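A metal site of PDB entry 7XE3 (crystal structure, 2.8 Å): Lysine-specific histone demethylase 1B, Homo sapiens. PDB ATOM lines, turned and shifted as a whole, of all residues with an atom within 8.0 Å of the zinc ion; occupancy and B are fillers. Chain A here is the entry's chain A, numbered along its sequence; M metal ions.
The zinc ion is bound by SG of Cys 63.
SG of Cys 44 is bound to the zinc ion (2.3 Å).
The zinc ion is bound by SG of Cys 36, at 2.3 Å.
The side-chain sulfur (SG) of Cys 66 is bound to the zinc ion (2.3 Å).
Residues that only touch the zinc ion: Ser 39 (3.9 Å) and Ala 45 (3.9 Å).
Six residues have an atom within 4 Å of the zinc ion: Cys 36, Ser 39, Cys 44, Ala 45, Cys 63 and Cys 66.
The nearest printed residue that does not touch the zinc ion is Lys 46 (4.7 Å).
SG of Cys 63 lies close to OE1 of Glu 65, 3.5 Å away.
SG of Cys 44 sits close to OG of Ser 39 (3.6 Å).
SG of Cys 36 lies close to N of Ala 38 (3.5 Å).
N of Cys 36 lies within hydrogen-bond range of O of Lys 46, at 2.7 Å.
The backbone NH (N) of Ser 39 sits close to the side-chain sulfur (SG) of Cys 36, 3.8 Å away.
N of Lys 46 lies close to SG of Cys 44 (3.2 Å).
The backbone NH of Ser 39 lies close to the side-chain sulfur of Cys 66, 3.5 Å away.
The backbone NH (N) of Ser 41 sits close to the side-chain sulfur (SG) of Cys 66.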
ATOM      1  N   VAL A  35       9.834   5.911 -28.380  1.00  0.00           N
ATOM      2  CA  VAL A  35       8.381   5.950 -28.416  1.00  0.00           C
ATOM      3  C   VAL A  35       7.892   6.027 -26.972  1.00  0.00           C
ATOM      4  O   VAL A  35       8.397   5.310 -26.103  1.00  0.00           O
ATOM      5  CB  VAL A  35       7.791   4.730 -29.134  1.00  0.00           C
ATOM      6  CG1 VAL A  35       8.452   4.571 -30.483  1.00  0.00           C
ATOM      7  CG2 VAL A  35       7.992   3.457 -28.337  1.00  0.00           C
ATOM      8  N   CYS A  36       6.951   6.918 -26.707  1.00  0.00           N
ATOM      9  CA  CYS A  36       6.552   7.149 -25.331  1.00  0.00           C
ATOM     10  C   CYS A  36       5.750   5.956 -24.824  1.00  0.00           C
ATOM     11  O   CYS A  36       4.736   5.577 -25.424  1.00  0.00           O
ATOM     12  CB  CYS A  36       5.737   8.428 -25.226  1.00  0.00           C
ATOM     13  SG  CYS A  36       5.484   8.885 -23.495  1.00  0.00           S
ATOM     14  N   PHE A  37       6.197   5.367 -23.714  1.00  0.00           N
ATOM     15  CA  PHE A  37       5.471   4.269 -23.106  1.00  0.00           C
ATOM     16  C   PHE A  37       4.295   4.736 -22.249  1.00  0.00           C
ATOM     17  O   PHE A  37       3.439   3.921 -21.904  1.00  0.00           O
ATOM     18  CB  PHE A  37       6.400   3.420 -22.237  1.00  0.00           C
ATOM     19  CG  PHE A  37       6.811   4.071 -20.937  1.00  0.00           C
ATOM     20  CD1 PHE A  37       5.941   4.125 -19.846  1.00  0.00           C
ATOM     21  CD2 PHE A  37       8.100   4.582 -20.782  1.00  0.00           C
ATOM     22  CE1 PHE A  37       6.317   4.707 -18.653  1.00  0.00           C
ATOM     23  CE2 PHE A  37       8.494   5.170 -19.573  1.00  0.00           C
ATOM     24  CZ  PHE A  37       7.600   5.227 -18.506  1.00  0.00           C
ATOM     25  N   ALA A  38       4.279   6.012 -21.860  1.00  0.00           N
ATOM     26  CA  ALA A  38       3.334   6.492 -20.862  1.00  0.00           C
ATOM     27  C   ALA A  38       1.994   6.854 -21.505  1.00  0.00           C
ATOM     28  O   ALA A  38       0.959   6.286 -21.143  1.00  0.00           O
ATOM     29  CB  ALA A  38       3.923   7.709 -20.135  1.00  0.00           C
ATOM     30  N   SER A  39       2.012   7.781 -22.456  1.00  0.00           N
ATOM     31  CA  SER A  39       0.788   8.315 -23.027  1.00  0.00           C
ATOM     32  C   SER A  39      -0.131   8.816 -21.920  1.00  0.00           C
ATOM     33  O   SER A  39      -1.327   8.534 -21.890  1.00  0.00           O
ATOM     34  CB  SER A  39       0.097   7.288 -23.929  1.00  0.00           C
ATOM     35  OG  SER A  39       0.761   7.191 -25.189  1.00  0.00           O
ATOM     36  N   ALA A  40       0.457   9.556 -20.990  1.00  0.00           N
ATOM     37  CA  ALA A  40      -0.270  10.137 -19.876  1.00  0.00           C
ATOM     38  C   ALA A  40      -0.878  11.488 -20.206  1.00  0.00           C
ATOM     39  O   ALA A  40      -1.909  11.850 -19.632  1.00  0.00           O
ATOM     40  CB  ALA A  40       0.651  10.272 -18.669  1.00  0.00           C
ATOM     41  N   SER A  41      -0.256  12.254 -21.104  1.00  0.00           N
ATOM     42  CA  SER A  41      -0.712  13.595 -21.455  1.00  0.00           C
ATOM     43  C   SER A  41      -1.552  13.566 -22.728  1.00  0.00           C
ATOM     44  O   SER A  41      -1.392  12.708 -23.587  1.00  0.00           O
ATOM     45  CB  SER A  41       0.466  14.548 -21.642  1.00  0.00           C
ATOM     46  OG  SER A  41       0.002  15.891 -21.821  1.00  0.00           O
ATOM     47  N   GLU A  42      -2.450  14.547 -22.822  1.00  0.00           N
ATOM     48  CA  GLU A  42      -3.237  14.706 -24.039  1.00  0.00           C
ATOM     49  C   GLU A  42      -2.369  14.959 -25.256  1.00  0.00           C
ATOM     50  O   GLU A  42      -2.746  14.610 -26.374  1.00  0.00           O
ATOM     51  CB  GLU A  42      -4.247  15.840 -23.858  1.00  0.00           C
ATOM     52  CG  GLU A  42      -5.186  15.649 -22.685  1.00  0.00           C
ATOM     53  CD  GLU A  42      -6.019  14.392 -22.821  1.00  0.00           C
ATOM     54  OE1 GLU A  42      -7.065  14.448 -23.515  1.00  0.00           O
ATOM     55  OE2 GLU A  42      -5.620  13.340 -22.255  1.00  0.00           O
ATOM     56  N   ARG A  43      -1.188  15.555 -25.055  1.00  0.00           N
ATOM     57  CA  ARG A  43      -0.281  15.916 -26.139  1.00  0.00           C
ATOM     58  C   ARG A  43       0.974  15.051 -26.148  1.00  0.00           C
ATOM     59  O   ARG A  43       2.043  15.514 -26.543  1.00  0.00           O
ATOM     60  CB  ARG A  43       0.122  17.387 -26.051  1.00  0.00           C
ATOM     61  CG  ARG A  43      -1.013  18.398 -26.141  1.00  0.00           C
ATOM     62  CD  ARG A  43      -0.489  19.794 -25.758  1.00  0.00           C
ATOM     63  NE  ARG A  43       0.442  19.674 -24.621  1.00  0.00           N
ATOM     64  CZ  ARG A  43       0.202  20.112 -23.391  1.00  0.00           C
ATOM     65  NH1 ARG A  43      -0.870  20.851 -23.107  1.00  0.00           N
ATOM     66  NH2 ARG A  43       1.065  19.814 -22.417  1.00  0.00           N
ATOM     67  N   CYS A  44       0.859  13.793 -25.690  1.00  0.00           N
ATOM     68  CA  CYS A  44       1.982  12.855 -25.758  1.00  0.00           C
ATOM     69  C   CYS A  44       2.618  12.907 -27.141  1.00  0.00           C
ATOM     70  O   CYS A  44       1.925  13.016 -28.156  1.00  0.00           O
ATOM     71  CB  CYS A  44       1.509  11.439 -25.439  1.00  0.00           C
ATOM     72  SG  CYS A  44       2.760  10.103 -25.718  1.00  0.00           S
ATOM     73  N   ALA A  45       3.951  12.829 -27.172  1.00  0.00           N
ATOM     74  CA  ALA A  45       4.684  12.848 -28.443  1.00  0.00           C
ATOM     75  C   ALA A  45       4.580  11.539 -29.209  1.00  0.00           C
ATOM     76  O   ALA A  45       5.095  11.457 -30.328  1.00  0.00           O
ATOM     77  CB  ALA A  45       6.150  13.183 -28.204  1.00  0.00           C
ATOM     78  N   LYS A  46       3.928  10.515 -28.648  1.00  0.00           N
ATOM     79  CA  LYS A  46       3.810   9.203 -29.277  1.00  0.00           C
ATOM     80  C   LYS A  46       5.183   8.678 -29.691  1.00  0.00           C
ATOM     81  O   LYS A  46       5.895   8.119 -28.860  1.00  0.00           O
ATOM     82  CB  LYS A  46       2.860   9.286 -30.473  1.00  0.00           C
ATOM     83  CG  LYS A  46       1.434   9.707 -30.095  1.00  0.00           C
ATOM     84  CD  LYS A  46       0.779   8.730 -29.129  1.00  0.00           C
ATOM     85  CE  LYS A  46      -0.709   9.051 -28.917  1.00  0.00           C
ATOM     86  NZ  LYS A  46      -1.328   8.197 -27.846  1.00  0.00           N
ATOM     87  N   ASN A  47       5.563   8.860 -30.973  1.00  0.00           N
ATOM     88  CA  ASN A  47       6.858   8.392 -31.465  1.00  0.00           C
ATOM     89  C   ASN A  47       7.596   9.434 -32.307  1.00  0.00           C
ATOM     90  O   ASN A  47       8.478   9.064 -33.103  1.00  0.00           O
ATOM     91  CB  ASN A  47       6.693   7.085 -32.251  1.00  0.00           C
ATOM     92  CG  ASN A  47       5.720   7.203 -33.428  1.00  0.00           C
ATOM     93  OD1 ASN A  47       5.448   8.291 -33.960  1.00  0.00           O
ATOM     94  ND2 ASN A  47       5.191   6.048 -33.854  1.00  0.00           N
ATOM     95  N   THR A  50       9.976  15.862 -29.426  1.00  0.00           N
ATOM     96  CA  THR A  50       9.628  16.416 -28.129  1.00  0.00           C
ATOM     97  C   THR A  50      10.803  17.244 -27.650  1.00  0.00           C
ATOM     98  O   THR A  50      11.915  17.127 -28.163  1.00  0.00           O
ATOM     99  CB  THR A  50       9.255  15.297 -27.145  1.00  0.00           C
ATOM    100  OG1 THR A  50       8.716  15.854 -25.944  1.00  0.00           O
ATOM    101  CG2 THR A  50      10.454  14.434 -26.828  1.00  0.00           C
ATOM    102  N   TRP A  53      13.542  13.693 -24.737  1.00  0.00           N
ATOM    103  CA  TRP A  53      13.151  12.289 -24.680  1.00  0.00           C
ATOM    104  C   TRP A  53      13.799  11.672 -23.439  1.00  0.00           C
ATOM    105  O   TRP A  53      14.974  11.301 -23.453  1.00  0.00           O
ATOM    106  CB  TRP A  53      13.565  11.566 -25.953  1.00  0.00           C
ATOM    107  CG  TRP A  53      12.507  11.565 -27.005  1.00  0.00           C
ATOM    108  CD1 TRP A  53      12.559  12.193 -28.222  1.00  0.00           C
ATOM    109  CD2 TRP A  53      11.235  10.912 -26.951  1.00  0.00           C
ATOM    110  NE1 TRP A  53      11.397  11.967 -28.931  1.00  0.00           N
ATOM    111  CE2 TRP A  53      10.566  11.184 -28.171  1.00  0.00           C
ATOM    112  CE3 TRP A  53      10.595  10.130 -25.997  1.00  0.00           C
ATOM    113  CZ2 TRP A  53       9.294  10.697 -28.455  1.00  0.00           C
ATOM    114  CZ3 TRP A  53       9.323   9.643 -26.281  1.00  0.00           C
ATOM    115  CH2 TRP A  53       8.688   9.930 -27.501  1.00  0.00           C
ATOM    116  N   HIS A  61      11.365   4.899 -23.049  1.00  0.00           N
ATOM    117  CA  HIS A  61      11.484   6.353 -22.982  1.00  0.00           C
ATOM    118  C   HIS A  61      10.096   6.960 -22.821  1.00  0.00           C
ATOM    119  O   HIS A  61       9.088   6.351 -23.181  1.00  0.00           O
ATOM    120  CB  HIS A  61      12.152   6.935 -24.231  1.00  0.00           C
ATOM    121  CG  HIS A  61      13.458   6.289 -24.571  1.00  0.00           C
ATOM    122  ND1 HIS A  61      13.545   5.009 -25.089  1.00  0.00           N
ATOM    123  CD2 HIS A  61      14.732   6.737 -24.484  1.00  0.00           C
ATOM    124  CE1 HIS A  61      14.810   4.703 -25.291  1.00  0.00           C
ATOM    125  NE2 HIS A  61      15.550   5.731 -24.930  1.00  0.00           N
ATOM    126  N   PHE A  62      10.067   8.183 -22.303  1.00  0.00           N
ATOM    127  CA  PHE A  62       8.820   8.935 -22.270  1.00  0.00           C
ATOM    128  C   PHE A  62       9.062  10.391 -22.613  1.00  0.00           C
ATOM    129  O   PHE A  62      10.110  10.957 -22.283  1.00  0.00           O
ATOM    130  CB  PHE A  62       8.108   8.830 -20.908  1.00  0.00           C
ATOM    131  CG  PHE A  62       8.927   9.312 -19.753  1.00  0.00           C
ATOM    132  CD1 PHE A  62       9.759   8.439 -19.070  1.00  0.00           C
ATOM    133  CD2 PHE A  62       8.848  10.635 -19.336  1.00  0.00           C
ATOM    134  CE1 PHE A  62      10.507   8.884 -18.005  1.00  0.00           C
ATOM    135  CE2 PHE A  62       9.604  11.074 -18.272  1.00  0.00           C
ATOM    136  CZ  PHE A  62      10.441  10.191 -17.603  1.00  0.00           C
ATOM    137  N   CYS A  63       8.084  10.989 -23.281  1.00  0.00           N
ATOM    138  CA  CYS A  63       8.163  12.329 -23.823  1.00  0.00           C
ATOM    139  C   CYS A  63       8.010  13.391 -22.737  1.00  0.00           C
ATOM    140  O   CYS A  63       7.542  13.143 -21.624  1.00  0.00           O
ATOM    141  CB  CYS A  63       7.098  12.528 -24.888  1.00  0.00           C
ATOM    142  SG  CYS A  63       5.459  12.520 -24.186  1.00  0.00           S
ATOM    143  N   ASN A  64       8.380  14.630 -23.084  1.00  0.00           N
ATOM    144  CA  ASN A  64       8.383  15.680 -22.074  1.00  0.00           C
ATOM    145  C   ASN A  64       6.965  16.112 -21.702  1.00  0.00           C
ATOM    146  O   ASN A  64       6.744  16.590 -20.583  1.00  0.00           O
ATOM    147  CB  ASN A  64       9.201  16.875 -22.556  1.00  0.00           C
ATOM    148  CG  ASN A  64       9.218  17.997 -21.550  1.00  0.00           C
ATOM    149  OD1 ASN A  64       9.830  17.869 -20.481  1.00  0.00           O
ATOM    150  ND2 ASN A  64       8.524  19.086 -21.872  1.00  0.00           N
ATOM    151  N   GLU A  65       6.012  15.964 -22.617  1.00  0.00           N
ATOM    152  CA  GLU A  65       4.633  16.300 -22.273  1.00  0.00           C
ATOM    153  C   GLU A  65       4.131  15.396 -21.147  1.00  0.00           C
ATOM    154  O   GLU A  65       3.597  15.880 -20.132  1.00  0.00           O
ATOM    155  CB  GLU A  65       3.744  16.198 -23.516  1.00  0.00           C
ATOM    156  CG  GLU A  65       4.049  17.250 -24.589  1.00  0.00           C
ATOM    157  CD  GLU A  65       5.295  16.929 -25.414  1.00  0.00           C
ATOM    158  OE1 GLU A  65       5.813  15.789 -25.291  1.00  0.00           O
ATOM    159  OE2 GLU A  65       5.766  17.811 -26.176  1.00  0.00           O
ATOM    160  N   CYS A  66       4.330  14.085 -21.280  1.00  0.00           N
ATOM    161  CA  CYS A  66       3.973  13.167 -20.210  1.00  0.00           C
ATOM    162  C   CYS A  66       4.810  13.438 -18.957  1.00  0.00           C
ATOM    163  O   CYS A  66       4.359  13.161 -17.840  1.00  0.00           O
ATOM    164  CB  CYS A  66       4.155  11.718 -20.666  1.00  0.00           C
ATOM    165  SG  CYS A  66       2.949  11.153 -21.906  1.00  0.00           S
ATOM    166  N   PHE A  67       6.025  13.972 -19.118  1.00  0.00           N
ATOM    167  CA  PHE A  67       6.810  14.373 -17.966  1.00  0.00           C
ATOM    168  C   PHE A  67       6.130  15.517 -17.220  1.00  0.00           C
ATOM    169  O   PHE A  67       6.031  15.495 -15.983  1.00  0.00           O
ATOM    170  CB  PHE A  67       8.227  14.762 -18.416  1.00  0.00           C
ATOM    171  CG  PHE A  67       9.089  15.345 -17.313  1.00  0.00           C
ATOM    172  CD1 PHE A  67       9.035  16.700 -16.999  1.00  0.00           C
ATOM    173  CD2 PHE A  67       9.994  14.541 -16.636  1.00  0.00           C
ATOM    174  CE1 PHE A  67       9.840  17.234 -16.011  1.00  0.00           C
ATOM    175  CE2 PHE A  67      10.808  15.073 -15.658  1.00  0.00           C
ATOM    176  CZ  PHE A  67      10.724  16.418 -15.331  1.00  0.00           C
ATOM    177  N   HIS A  69       2.987  16.184 -17.353  1.00  0.00           N
ATOM    178  CA  HIS A  69       1.660  15.766 -16.899  1.00  0.00           C
ATOM    179  C   HIS A  69       1.666  15.494 -15.402  1.00  0.00           C
ATOM    180  O   HIS A  69       0.728  15.883 -14.695  1.00  0.00           O
ATOM    181  CB  HIS A  69       1.208  14.524 -17.677  1.00  0.00           C
ATOM    182  CG  HIS A  69      -0.194  14.087 -17.372  1.00  0.00           C
ATOM    183  ND1 HIS A  69      -0.481  12.965 -16.623  1.00  0.00           N
ATOM    184  CD2 HIS A  69      -1.390  14.614 -17.725  1.00  0.00           C
ATOM    185  CE1 HIS A  69      -1.788  12.828 -16.527  1.00  0.00           C
ATOM    186  NE2 HIS A  69      -2.362  13.819 -17.188  1.00  0.00           N
ATOM    187  N   MET A 102       7.823   6.931 -12.821  1.00  0.00           N
ATOM    188  CA  MET A 102       7.453   6.149 -14.000  1.00  0.00           C
ATOM    189  C   MET A 102       7.847   4.693 -13.841  1.00  0.00           C
ATOM    190  O   MET A 102       7.040   3.780 -14.084  1.00  0.00           O
ATOM    191  CB  MET A 102       8.115   6.723 -15.253  1.00  0.00           C
ATOM    192  CG  MET A 102       7.608   8.077 -15.716  1.00  0.00           C
ATOM    193  SD  MET A 102       5.872   8.066 -16.173  1.00  0.00           S
ATOM    194  CE  MET A 102       5.773   9.615 -17.057  1.00  0.00           C
HETATM  195 ZN    ZN M   1       4.083  10.690 -23.911  1.00  0.00          ZN
